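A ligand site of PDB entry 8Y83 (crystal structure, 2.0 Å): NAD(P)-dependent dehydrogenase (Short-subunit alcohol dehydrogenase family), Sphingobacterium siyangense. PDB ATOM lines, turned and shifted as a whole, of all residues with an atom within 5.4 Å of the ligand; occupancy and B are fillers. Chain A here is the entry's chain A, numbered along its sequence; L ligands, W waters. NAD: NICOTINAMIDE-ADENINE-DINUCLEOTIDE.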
ATOM      1  N   THR A  12      29.506   4.223  23.046  1.00  0.00           N
ATOM      2  CA  THR A  12      29.072   4.751  21.754  1.00  0.00           C
ATOM      3  C   THR A  12      27.923   3.876  21.230  1.00  0.00           C
ATOM      4  O   THR A  12      27.827   2.680  21.567  1.00  0.00           O
ATOM      5  CB  THR A  12      30.213   4.832  20.740  1.00  0.00           C
ATOM      6  OG1 THR A  12      30.642   3.519  20.332  1.00  0.00           O
ATOM      7  CG2 THR A  12      31.384   5.628  21.288  1.00  0.00           C
ATOM      8  N   GLY A  13      27.011   4.514  20.470  1.00  0.00           N
ATOM      9  CA  GLY A  13      25.798   3.885  19.950  1.00  0.00           C
ATOM     10  C   GLY A  13      24.918   3.298  21.038  1.00  0.00           C
ATOM     11  O   GLY A  13      24.342   2.220  20.846  1.00  0.00           O
ATOM     12  N   SER A  14      24.792   4.005  22.166  1.00  0.00           N
ATOM     13  CA  SER A  14      24.060   3.539  23.331  1.00  0.00           C
ATOM     14  C   SER A  14      22.602   4.028  23.321  1.00  0.00           C
ATOM     15  O   SER A  14      21.852   3.802  24.279  1.00  0.00           O
ATOM     16  CB  SER A  14      24.771   3.927  24.620  1.00  0.00           C
ATOM     17  OG  SER A  14      25.468   5.150  24.433  1.00  0.00           O
ATOM     18  N   GLY A  15      22.168   4.532  22.162  1.00  0.00           N
ATOM     19  CA  GLY A  15      20.773   4.951  22.007  1.00  0.00           C
ATOM     20  C   GLY A  15      19.819   3.764  21.925  1.00  0.00           C
ATOM     21  O   GLY A  15      18.652   3.909  22.247  1.00  0.00           O
ATOM     22  N   SER A  16      20.332   2.583  21.517  1.00  0.00           N
ATOM     23  CA  SER A  16      19.511   1.446  21.143  1.00  0.00           C
ATOM     24  C   SER A  16      20.304   0.146  21.267  1.00  0.00           C
ATOM     25  O   SER A  16      21.522   0.160  21.278  1.00  0.00           O
ATOM     26  CB  SER A  16      19.013   1.667  19.721  1.00  0.00           C
ATOM     27  OG  SER A  16      18.770   0.432  19.073  1.00  0.00           O
ATOM     28  N   GLY A  17      19.600  -0.987  21.388  1.00  0.00           N
ATOM     29  CA  GLY A  17      20.180  -2.296  21.167  1.00  0.00           C
ATOM     30  C   GLY A  17      21.207  -2.712  22.228  1.00  0.00           C
ATOM     31  O   GLY A  17      20.992  -2.600  23.448  1.00  0.00           O
ATOM     32  N   ILE A  18      22.323  -3.239  21.742  1.00  0.00           N
ATOM     33  CA  ILE A  18      23.383  -3.712  22.618  1.00  0.00           C
ATOM     34  C   ILE A  18      23.939  -2.547  23.448  1.00  0.00           C
ATOM     35  O   ILE A  18      24.188  -2.711  24.646  1.00  0.00           O
ATOM     36  CB  ILE A  18      24.464  -4.469  21.827  1.00  0.00           C
ATOM     37  CG1 ILE A  18      23.897  -5.805  21.267  1.00  0.00           C
ATOM     38  CG2 ILE A  18      25.720  -4.735  22.668  1.00  0.00           C
ATOM     39  CD1 ILE A  18      24.824  -6.521  20.290  1.00  0.00           C
ATOM     40  N   GLY A  19      24.159  -1.404  22.805  1.00  0.00           N
ATOM     41  CA  GLY A  19      24.744  -0.230  23.450  1.00  0.00           C
ATOM     42  C   GLY A  19      23.877   0.222  24.626  1.00  0.00           C
ATOM     43  O   GLY A  19      24.399   0.555  25.695  1.00  0.00           O
ATOM     44  N   SER A  36      26.603   8.241  24.058  1.00  0.00           N
ATOM     45  CA  SER A  36      26.791   8.904  22.775  1.00  0.00           C
ATOM     46  C   SER A  36      26.013   8.172  21.681  1.00  0.00           C
ATOM     47  O   SER A  36      25.977   6.942  21.608  1.00  0.00           O
ATOM     48  CB  SER A  36      28.249   9.000  22.413  1.00  0.00           C
ATOM     49  OG  SER A  36      28.400   9.908  21.336  1.00  0.00           O
ATOM     50  N   ASP A  37      25.446   8.954  20.772  1.00  0.00           N
ATOM     51  CA  ASP A  37      24.683   8.393  19.671  1.00  0.00           C
ATOM     52  C   ASP A  37      24.452   9.502  18.639  1.00  0.00           C
ATOM     53  O   ASP A  37      24.670  10.669  18.927  1.00  0.00           O
ATOM     54  CB  ASP A  37      23.364   7.781  20.133  1.00  0.00           C
ATOM     55  CG  ASP A  37      22.854   6.684  19.207  1.00  0.00           C
ATOM     56  OD1 ASP A  37      22.574   6.993  18.015  1.00  0.00           O
ATOM     57  OD2 ASP A  37      22.812   5.507  19.656  1.00  0.00           O
ATOM     58  N   ILE A  38      24.111   9.072  17.428  1.00  0.00           N
ATOM     59  CA  ILE A  38      23.689   9.921  16.324  1.00  0.00           C
ATOM     60  C   ILE A  38      22.285  10.440  16.623  1.00  0.00           C
ATOM     61  O   ILE A  38      21.943  11.517  16.182  1.00  0.00           O
ATOM     62  CB  ILE A  38      23.714   9.066  15.025  1.00  0.00           C
ATOM     63  CG1 ILE A  38      25.015   9.201  14.320  1.00  0.00           C
ATOM     64  CG2 ILE A  38      22.550   9.362  14.089  1.00  0.00           C
ATOM     65  CD1 ILE A  38      25.660  10.554  14.480  1.00  0.00           C
ATOM     66  N   ASN A  39      21.476   9.640  17.327  1.00  0.00           N
ATOM     67  CA  ASN A  39      20.086   9.971  17.583  1.00  0.00           C
ATOM     68  C   ASN A  39      19.876  10.489  19.005  1.00  0.00           C
ATOM     69  O   ASN A  39      19.926   9.723  19.979  1.00  0.00           O
ATOM     70  CB  ASN A  39      19.185   8.768  17.322  1.00  0.00           C
ATOM     71  CG  ASN A  39      17.747   9.045  17.702  1.00  0.00           C
ATOM     72  OD1 ASN A  39      17.359  10.178  18.016  1.00  0.00           O
ATOM     73  ND2 ASN A  39      16.946   8.002  17.706  1.00  0.00           N
ATOM     74  N   ALA A  42      16.831   9.034  21.174  1.00  0.00           N
ATOM     75  CA  ALA A  42      17.225   7.731  21.700  1.00  0.00           C
ATOM     76  C   ALA A  42      18.215   7.912  22.859  1.00  0.00           C
ATOM     77  O   ALA A  42      18.049   7.304  23.922  1.00  0.00           O
ATOM     78  CB  ALA A  42      17.789   6.880  20.568  1.00  0.00           C
ATOM     79  N   ALA A  62      27.396  12.508  18.959  1.00  0.00           N
ATOM     80  CA  ALA A  62      28.633  12.344  18.232  1.00  0.00           C
ATOM     81  C   ALA A  62      28.444  11.304  17.142  1.00  0.00           C
ATOM     82  O   ALA A  62      27.744  10.304  17.347  1.00  0.00           O
ATOM     83  CB  ALA A  62      29.775  11.921  19.140  1.00  0.00           C
ATOM     84  N   ASP A  63      29.059  11.577  16.007  1.00  0.00           N
ATOM     85  CA  ASP A  63      29.244  10.590  14.960  1.00  0.00           C
ATOM     86  C   ASP A  63      30.589   9.888  15.159  1.00  0.00           C
ATOM     87  O   ASP A  63      31.637  10.529  15.078  1.00  0.00           O
ATOM     88  CB  ASP A  63      29.141  11.269  13.611  1.00  0.00           C
ATOM     89  CG  ASP A  63      29.387  10.392  12.400  1.00  0.00           C
ATOM     90  OD1 ASP A  63      29.649   9.175  12.545  1.00  0.00           O
ATOM     91  OD2 ASP A  63      29.336  10.953  11.316  1.00  0.00           O
ATOM     92  N   SER A  64      30.529   8.571  15.364  1.00  0.00           N
ATOM     93  CA  SER A  64      31.666   7.719  15.685  1.00  0.00           C
ATOM     94  C   SER A  64      32.706   7.739  14.576  1.00  0.00           C
ATOM     95  O   SER A  64      33.887   7.492  14.818  1.00  0.00           O
ATOM     96  CB  SER A  64      31.216   6.283  15.944  1.00  0.00           C
ATOM     97  OG  SER A  64      30.796   6.164  17.287  1.00  0.00           O
ATOM     98  N   SER A  65      32.266   8.002  13.341  1.00  0.00           N
ATOM     99  CA  SER A  65      33.191   8.047  12.211  1.00  0.00           C
ATOM    100  C   SER A  65      34.023   9.331  12.157  1.00  0.00           C
ATOM    101  O   SER A  65      34.957   9.397  11.365  1.00  0.00           O
ATOM    102  CB  SER A  65      32.471   7.860  10.896  1.00  0.00           C
ATOM    103  OG  SER A  65      31.623   8.966  10.630  1.00  0.00           O
ATOM    104  N   ASN A  90      30.862   0.652  20.602  1.00  0.00           N
ATOM    105  CA  ASN A  90      29.756  -0.188  20.224  1.00  0.00           C
ATOM    106  C   ASN A  90      29.097   0.303  18.944  1.00  0.00           C
ATOM    107  O   ASN A  90      28.466  -0.493  18.283  1.00  0.00           O
ATOM    108  CB  ASN A  90      28.794  -0.374  21.379  1.00  0.00           C
ATOM    109  CG  ASN A  90      27.433  -0.858  20.943  1.00  0.00           C
ATOM    110  OD1 ASN A  90      27.168  -2.069  20.910  1.00  0.00           O
ATOM    111  ND2 ASN A  90      26.557   0.055  20.564  1.00  0.00           N
ATOM    112  N   ALA A  91      29.214   1.581  18.598  1.00  0.00           N
ATOM    113  CA  ALA A  91      28.473   2.130  17.467  1.00  0.00           C
ATOM    114  C   ALA A  91      28.831   1.329  16.220  1.00  0.00           C
ATOM    115  O   ALA A  91      29.989   1.056  16.018  1.00  0.00           O
ATOM    116  CB  ALA A  91      28.773   3.626  17.269  1.00  0.00           C
ATOM    117  N   GLY A  92      27.839   0.922  15.431  1.00  0.00           N
ATOM    118  CA  GLY A  92      28.077   0.157  14.221  1.00  0.00           C
ATOM    119  C   GLY A  92      26.825   0.046  13.368  1.00  0.00           C
ATOM    120  O   GLY A  92      25.730   0.179  13.879  1.00  0.00           O
ATOM    121  N   ILE A  93      27.026  -0.232  12.075  1.00  0.00           N
ATOM    122  CA  ILE A  93      25.944  -0.526  11.147  1.00  0.00           C
ATOM    123  C   ILE A  93      26.212  -1.896  10.496  1.00  0.00           C
ATOM    124  O   ILE A  93      27.332  -2.367  10.442  1.00  0.00           O
ATOM    125  CB  ILE A  93      25.817   0.585  10.078  1.00  0.00           C
ATOM    126  CG1 ILE A  93      27.089   0.734   9.265  1.00  0.00           C
ATOM    127  CG2 ILE A  93      25.370   1.934  10.686  1.00  0.00           C
ATOM    128  CD1 ILE A  93      26.848   1.452   7.955  1.00  0.00           C
ATOM    129  N   ILE A 114      32.545   3.757   9.901  1.00  0.00           N
ATOM    130  CA  ILE A 114      31.862   3.678  11.180  1.00  0.00           C
ATOM    131  C   ILE A 114      32.390   2.504  12.034  1.00  0.00           C
ATOM    132  O   ILE A 114      32.662   2.678  13.223  1.00  0.00           O
ATOM    133  CB  ILE A 114      30.336   3.596  10.962  1.00  0.00           C
ATOM    134  CG1 ILE A 114      29.789   4.864  10.306  1.00  0.00           C
ATOM    135  CG2 ILE A 114      29.598   3.284  12.272  1.00  0.00           C
ATOM    136  CD1 ILE A 114      28.372   4.709   9.784  1.00  0.00           C
ATOM    137  N   ASN A 115      32.475   1.301  11.429  1.00  0.00           N
ATOM    138  CA  ASN A 115      32.669   0.060  12.167  1.00  0.00           C
ATOM    139  C   ASN A 115      34.142  -0.168  12.471  1.00  0.00           C
ATOM    140  O   ASN A 115      34.448  -0.990  13.317  1.00  0.00           O
ATOM    141  CB  ASN A 115      32.119  -1.178  11.454  1.00  0.00           C
ATOM    142  CG  ASN A 115      30.607  -1.190  11.381  1.00  0.00           C
ATOM    143  OD1 ASN A 115      29.941  -0.160  11.558  1.00  0.00           O
ATOM    144  ND2 ASN A 115      30.006  -2.336  11.121  1.00  0.00           N
ATOM    145  N   MET A 141      33.388  -3.596  20.421  1.00  0.00           N
ATOM    146  CA  MET A 141      32.322  -4.481  19.997  1.00  0.00           C
ATOM    147  C   MET A 141      32.668  -5.043  18.618  1.00  0.00           C
ATOM    148  O   MET A 141      32.656  -4.336  17.600  1.00  0.00           O
ATOM    149  CB  MET A 141      30.961  -3.796  19.920  1.00  0.00           C
ATOM    150  CG  MET A 141      29.804  -4.796  19.794  1.00  0.00           C
ATOM    151  SD  MET A 141      29.585  -5.893  21.218  1.00  0.00           S
ATOM    152  CE  MET A 141      29.846  -4.695  22.543  1.00  0.00           C
ATOM    153  N   ALA A 142      33.026  -6.322  18.575  1.00  0.00           N
ATOM    154  CA  ALA A 142      33.266  -6.956  17.292  1.00  0.00           C
ATOM    155  C   ALA A 142      32.017  -7.752  16.931  1.00  0.00           C
ATOM    156  O   ALA A 142      30.895  -7.218  16.970  1.00  0.00           O
ATOM    157  CB  ALA A 142      34.551  -7.744  17.334  1.00  0.00           C
ATOM    158  N   SER A 143      32.191  -9.020  16.558  1.00  0.00           N
ATOM    159  CA  SER A 143      31.135  -9.894  16.085  1.00  0.00           C
ATOM    160  C   SER A 143      31.717 -11.290  15.945  1.00  0.00           C
ATOM    161  O   SER A 143      32.937 -11.427  15.895  1.00  0.00           O
ATOM    162  CB  SER A 143      30.565  -9.379  14.752  1.00  0.00           C
ATOM    163  OG  SER A 143      29.773 -10.356  14.067  1.00  0.00           O
ATOM    164  N   ILE A 144      30.844 -12.300  15.797  1.00  0.00           N
ATOM    165  CA  ILE A 144      31.245 -13.572  15.239  1.00  0.00           C
ATOM    166  C   ILE A 144      31.955 -13.338  13.917  1.00  0.00           C
ATOM    167  O   ILE A 144      32.837 -14.135  13.594  1.00  0.00           O
ATOM    168  CB  ILE A 144      30.084 -14.566  15.063  1.00  0.00           C
ATOM    169  CG1 ILE A 144      28.921 -13.928  14.336  1.00  0.00           C
ATOM    170  CG2 ILE A 144      29.675 -15.093  16.427  1.00  0.00           C
ATOM    171  CD1 ILE A 144      27.831 -14.881  13.844  1.00  0.00           C
ATOM    172  N   TYR A 156      31.325  -5.549   6.433  1.00  0.00           N
ATOM    173  CA  TYR A 156      31.084  -5.805   7.839  1.00  0.00           C
ATOM    174  C   TYR A 156      32.134  -6.802   8.388  1.00  0.00           C
ATOM    175  O   TYR A 156      32.797  -6.507   9.389  1.00  0.00           O
ATOM    176  CB  TYR A 156      29.648  -6.323   8.014  1.00  0.00           C
ATOM    177  CG  TYR A 156      29.191  -6.465   9.469  1.00  0.00           C
ATOM    178  CD1 TYR A 156      28.652  -5.389  10.170  1.00  0.00           C
ATOM    179  CD2 TYR A 156      29.289  -7.680  10.143  1.00  0.00           C
ATOM    180  CE1 TYR A 156      28.278  -5.510  11.512  1.00  0.00           C
ATOM    181  CE2 TYR A 156      28.874  -7.821  11.456  1.00  0.00           C
ATOM    182  CZ  TYR A 156      28.359  -6.743  12.149  1.00  0.00           C
ATOM    183  OH  TYR A 156      27.924  -6.854  13.451  1.00  0.00           O
ATOM    184  N   LYS A 160      35.020  -5.944  11.169  1.00  0.00           N
ATOM    185  CA  LYS A 160      34.984  -6.623  12.467  1.00  0.00           C
ATOM    186  C   LYS A 160      36.273  -7.410  12.705  1.00  0.00           C
ATOM    187  O   LYS A 160      36.756  -7.466  13.840  1.00  0.00           O
ATOM    188  CB  LYS A 160      33.734  -7.489  12.562  1.00  0.00           C
ATOM    189  CG  LYS A 160      32.461  -6.697  12.588  1.00  0.00           C
ATOM    190  CD  LYS A 160      32.372  -5.663  13.696  1.00  0.00           C
ATOM    191  CE  LYS A 160      30.990  -5.156  13.923  1.00  0.00           C
ATOM    192  NZ  LYS A 160      30.899  -4.299  15.133  1.00  0.00           N
ATOM    193  N   PRO A 186      29.613 -11.024  19.539  1.00  0.00           N
ATOM    194  CA  PRO A 186      28.278 -11.587  19.614  1.00  0.00           C
ATOM    195  C   PRO A 186      27.848 -12.345  18.364  1.00  0.00           C
ATOM    196  O   PRO A 186      28.183 -11.993  17.231  1.00  0.00           O
ATOM    197  CB  PRO A 186      27.374 -10.372  19.844  1.00  0.00           C
ATOM    198  CG  PRO A 186      28.343  -9.298  20.292  1.00  0.00           C
ATOM    199  CD  PRO A 186      29.587  -9.558  19.455  1.00  0.00           C
ATOM    200  N   GLY A 187      27.065 -13.401  18.618  1.00  0.00           N
ATOM    201  CA  GLY A 187      26.281 -14.021  17.563  1.00  0.00           C
ATOM    202  C   GLY A 187      25.073 -13.152  17.264  1.00  0.00           C
ATOM    203  O   GLY A 187      25.057 -11.984  17.637  1.00  0.00           O
ATOM    204  N   TYR A 188      24.043 -13.744  16.650  1.00  0.00           N
ATOM    205  CA  TYR A 188      22.860 -12.978  16.254  1.00  0.00           C
ATOM    206  C   TYR A 188      22.000 -12.723  17.472  1.00  0.00           C
ATOM    207  O   TYR A 188      21.619 -13.642  18.219  1.00  0.00           O
ATOM    208  CB  TYR A 188      22.161 -13.631  15.074  1.00  0.00           C
ATOM    209  CG  TYR A 188      22.924 -13.439  13.774  1.00  0.00           C
ATOM    210  CD1 TYR A 188      22.710 -12.328  12.953  1.00  0.00           C
ATOM    211  CD2 TYR A 188      23.911 -14.340  13.391  1.00  0.00           C
ATOM    212  CE1 TYR A 188      23.453 -12.117  11.803  1.00  0.00           C
ATOM    213  CE2 TYR A 188      24.620 -14.171  12.219  1.00  0.00           C
ATOM    214  CZ  TYR A 188      24.377 -13.067  11.411  1.00  0.00           C
ATOM    215  OH  TYR A 188      25.129 -12.892  10.307  1.00  0.00           O
ATOM    216  N   ILE A 189      21.644 -11.451  17.633  1.00  0.00           N
ATOM    217  CA  ILE A 189      21.003 -10.997  18.836  1.00  0.00           C
ATOM    218  C   ILE A 189      19.623 -10.470  18.463  1.00  0.00           C
ATOM    219  O   ILE A 189      19.462  -9.827  17.432  1.00  0.00           O
ATOM    220  CB  ILE A 189      21.837  -9.904  19.546  1.00  0.00           C
ATOM    221  CG1 ILE A 189      23.261 -10.333  19.863  1.00  0.00           C
ATOM    222  CG2 ILE A 189      21.107  -9.417  20.800  1.00  0.00           C
ATOM    223  CD1 ILE A 189      23.368 -11.599  20.690  1.00  0.00           C
ATOM    224  N   THR A 191      17.295  -7.950  18.257  1.00  0.00           N
ATOM    225  CA  THR A 191      17.076  -6.522  18.291  1.00  0.00           C
ATOM    226  C   THR A 191      15.777  -6.185  17.550  1.00  0.00           C
ATOM    227  O   THR A 191      15.128  -7.078  16.975  1.00  0.00           O
ATOM    228  CB  THR A 191      18.285  -5.803  17.680  1.00  0.00           C
ATOM    229  OG1 THR A 191      18.795  -6.601  16.620  1.00  0.00           O
ATOM    230  CG2 THR A 191      19.431  -5.621  18.650  1.00  0.00           C
ATOM    231  N   PRO A 192      15.332  -4.908  17.549  1.00  0.00           N
ATOM    232  CA  PRO A 192      14.242  -4.473  16.675  1.00  0.00           C
ATOM    233  C   PRO A 192      14.616  -4.569  15.196  1.00  0.00           C
ATOM    234  O   PRO A 192      13.767  -4.961  14.388  1.00  0.00           O
ATOM    235  CB  PRO A 192      13.973  -3.015  17.109  1.00  0.00           C
ATOM    236  CG  PRO A 192      14.666  -2.862  18.450  1.00  0.00           C
ATOM    237  CD  PRO A 192      15.847  -3.818  18.405  1.00  0.00           C
ATOM    238  N   LEU A 193      15.879  -4.232  14.848  1.00  0.00           N
ATOM    239  CA  LEU A 193      16.392  -4.361  13.476  1.00  0.00           C
ATOM    240  C   LEU A 193      16.191  -5.787  12.932  1.00  0.00           C
ATOM    241  O   LEU A 193      15.953  -5.968  11.739  1.00  0.00           O
ATOM    242  CB  LEU A 193      17.848  -3.905  13.339  1.00  0.00           C
ATOM    243  CG  LEU A 193      18.868  -4.455  14.345  1.00  0.00           C
ATOM    244  CD1 LEU A 193      20.233  -4.810  13.767  1.00  0.00           C
ATOM    245  CD2 LEU A 193      19.086  -3.458  15.465  1.00  0.00           C
ATOM    246  N   LEU A 194      16.272  -6.787  13.823  1.00  0.00           N
ATOM    247  CA  LEU A 194      16.113  -8.201  13.455  1.00  0.00           C
ATOM    248  C   LEU A 194      14.659  -8.472  13.050  1.00  0.00           C
ATOM    249  O   LEU A 194      14.389  -9.343  12.223  1.00  0.00           O
ATOM    250  CB  LEU A 194      16.541  -9.055  14.648  1.00  0.00           C
ATOM    251  CG  LEU A 194      17.505 -10.220  14.390  1.00  0.00           C
ATOM    252  CD1 LEU A 194      16.873 -11.300  13.516  1.00  0.00           C
ATOM    253  CD2 LEU A 194      18.835  -9.739  13.791  1.00  0.00           C
HETATM  254  PA  NAD L   1      21.250  -1.082  16.669  1.00  0.00           P
HETATM  255  O1A NAD L   1      21.092  -0.524  15.293  1.00  0.00           O
HETATM  256  O2A NAD L   1      20.116  -1.567  17.496  1.00  0.00           O
HETATM  257  O5B NAD L   1      22.089  -0.047  17.576  1.00  0.00           O
HETATM  258  C5B NAD L   1      23.073   0.752  16.906  1.00  0.00           C
HETATM  259  C4B NAD L   1      23.143   2.109  17.541  1.00  0.00           C
HETATM  260  O4B NAD L   1      24.312   2.771  17.007  1.00  0.00           O
HETATM  261  C3B NAD L   1      21.941   3.033  17.260  1.00  0.00           C
HETATM  262  O3B NAD L   1      21.512   3.714  18.428  1.00  0.00           O
HETATM  263  C2B NAD L   1      22.493   3.952  16.151  1.00  0.00           C
HETATM  264  O2B NAD L   1      21.837   5.202  16.083  1.00  0.00           O
HETATM  265  C1B NAD L   1      23.947   4.074  16.616  1.00  0.00           C
HETATM  266  N9A NAD L   1      24.861   4.537  15.597  1.00  0.00           N
HETATM  267  C8A NAD L   1      24.932   4.111  14.292  1.00  0.00           C
HETATM  268  N7A NAD L   1      25.862   4.731  13.598  1.00  0.00           N
HETATM  269  C5A NAD L   1      26.416   5.639  14.494  1.00  0.00           C
HETATM  270  C6A NAD L   1      27.432   6.602  14.347  1.00  0.00           C
HETATM  271  N6A NAD L   1      28.077   6.819  13.215  1.00  0.00           N
HETATM  272  N1A NAD L   1      27.752   7.341  15.442  1.00  0.00           N
HETATM  273  C2A NAD L   1      27.076   7.117  16.587  1.00  0.00           C
HETATM  274  N3A NAD L   1      26.092   6.254  16.822  1.00  0.00           N
HETATM  275  C4A NAD L   1      25.801   5.539  15.727  1.00  0.00           C
HETATM  276  O3  NAD L   1      22.338  -2.267  16.529  1.00  0.00           O
HETATM  277  PN  NAD L   1      23.019  -3.264  17.601  1.00  0.00           P
HETATM  278  O1N NAD L   1      22.597  -4.650  17.209  1.00  0.00           O
HETATM  279  O2N NAD L   1      22.776  -2.847  19.003  1.00  0.00           O
HETATM  280  O5D NAD L   1      24.568  -3.048  17.220  1.00  0.00           O
HETATM  281  C5D NAD L   1      25.558  -2.636  18.184  1.00  0.00           C
HETATM  282  C4D NAD L   1      26.883  -3.276  17.865  1.00  0.00           C
HETATM  283  O4D NAD L   1      26.793  -4.711  18.036  1.00  0.00           O
HETATM  284  C3D NAD L   1      27.420  -3.034  16.429  1.00  0.00           C
HETATM  285  O3D NAD L   1      28.819  -2.743  16.482  1.00  0.00           O
HETATM  286  C2D NAD L   1      27.114  -4.367  15.746  1.00  0.00           C
HETATM  287  O2D NAD L   1      28.004  -4.591  14.673  1.00  0.00           O
HETATM  288  C1D NAD L   1      27.364  -5.338  16.901  1.00  0.00           C
HETATM  289  N1N NAD L   1      26.756  -6.688  16.749  1.00  0.00           N
HETATM  290  C2N NAD L   1      25.382  -6.856  16.709  1.00  0.00           C
HETATM  291  C3N NAD L   1      24.839  -8.125  16.510  1.00  0.00           C
HETATM  292  C7N NAD L   1      23.351  -8.283  16.422  1.00  0.00           C
HETATM  293  O7N NAD L   1      22.608  -7.313  16.669  1.00  0.00           O
HETATM  294  N7N NAD L   1      22.876  -9.449  16.026  1.00  0.00           N
HETATM  295  C4N NAD L   1      25.670  -9.235  16.445  1.00  0.00           C
HETATM  296  C5N NAD L   1      27.031  -9.063  16.524  1.00  0.00           C
HETATM  297  C6N NAD L   1      27.564  -7.790  16.665  1.00  0.00           C
HETATM  298  O   HOH W   1      23.619  -0.692  19.989  1.00  0.00           O
HETATM  299  O   HOH W   2      22.818   0.038  13.428  1.00  0.00           O
HETATM  300  O   HOH W   3      31.526  -0.986  17.040  1.00  0.00           O
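The side-chain carboxylate (OD2) of Asp 37 is in hydrogen-bond range of an oxygen (O3B) of the ligand (2.5 Å). The side-chain hydroxyl (OH) of Tyr 156 is in hydrogen-bond range of an oxygen (O2D) of the ligand (2.6 Å). The backbone NH (N) of Ile 18 is in hydrogen-bond range of an oxygen (O2N) of the ligand (2.8 Å). The backbone NH of Ser 16 lies close to an oxygen (O3B) of the ligand, at 3.5 Å. The side-chain hydroxyl of Ser 16 lies within hydrogen-bond range of an oxygen (O2A) of the ligand, at 2.9 Å. O of Asn 90 is in hydrogen-bond range of O3D of the ligand (2.9 Å). N6A of the ligand sits at hydrogen-bond distance from OD1 of Asp 63 (2.9 Å). The side-chain amino group (NZ) of Lys 160 sits at hydrogen-bond distance from an oxygen (O3D) of the ligand (2.9 Å). The backbone NH (N) of Ser 64 is in hydrogen-bond range of a nitrogen (N1A) of the ligand (3.0 Å). N3A of the ligand sits at hydrogen-bond distance from N of Ile 38 (3.5 Å).
N of Ala 62 is in hydrogen-bond range of O of Asp 37 (3.3 Å). OD1 of Asp 37 sits at hydrogen-bond distance from N of Asn 39, 2.9 Å away. ND2 of Asn 90 is in hydrogen-bond range of O of Gly 13 (3.1 Å). N of Asn 90 lies within hydrogen-bond range of OG1 of Thr 12, at 2.9 Å. OD1 of Asp 63 lies within hydrogen-bond range of OG of Ser 65 (2.8 Å). NZ of Lys 160 sits at hydrogen-bond distance from O of Met 141 (3.0 Å). The backbone NH (N) of Ile 144 lies within hydrogen-bond range of the backbone carbonyl oxygen (O) of Pro 186 (3.0 Å). The backbone NH (N) of Gly 13 is in hydrogen-bond range of the backbone carbonyl oxygen (O) of Ser 36 (2.9 Å).
N7N of the ligand lies close to N of Ile 189 (2.8 Å). Gly 13 touches the ligand (CA to O4B, 3.5 Å). Gly 15 touches the ligand. Gly 17 touches the ligand (CA to O2N, 3.4 Å). O of Ala 62 touches C2A of the ligand, 3.3 Å away. Ala 91 touches the ligand (CB to N3A, 3.8 Å). Gly 92 touches the ligand. CG1 of Ile 114 touches N6A of the ligand, 3.9 Å away. Met 141 touches the ligand. Ala 142 touches the ligand. CB of Ser 143 touches C6N of the ligand, at 3.9 Å. O of Pro 186 touches C5N of the ligand, 3.2 Å away. O of Gly 187 touches C4N of the ligand, at 3.1 Å. Tyr 188 touches the ligand. CG2 of Thr 191 touches O1N of the ligand, at 3.6 Å. Leu 193 touches the ligand (CD2 to O2A, 3.0 Å). Hydrophobic or aromatic side chains that line the ligand: Ile 18, Ile 38, Ala 91, Ile 114, Met 141, Tyr 156, Pro 186, Ile 189 and Leu 193. Of the 37 residues printed, 25 come within 4 Å of the ligand. The nearest printed residue that does not touch the ligand is Ile 93 (4.1 Å).
Water W2 lies within hydrogen-bond range of O1A of the ligand (2.6 Å) and O of Gly 92 (3.0 Å). Water W3 lies within hydrogen-bond range of the backbone carbonyl oxygen (O) of Ala 91 (2.8 Å), an oxygen (O3D) of the ligand (3.3 Å) and the backbone carbonyl oxygen (O) of Asn 90 (3.3 Å).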
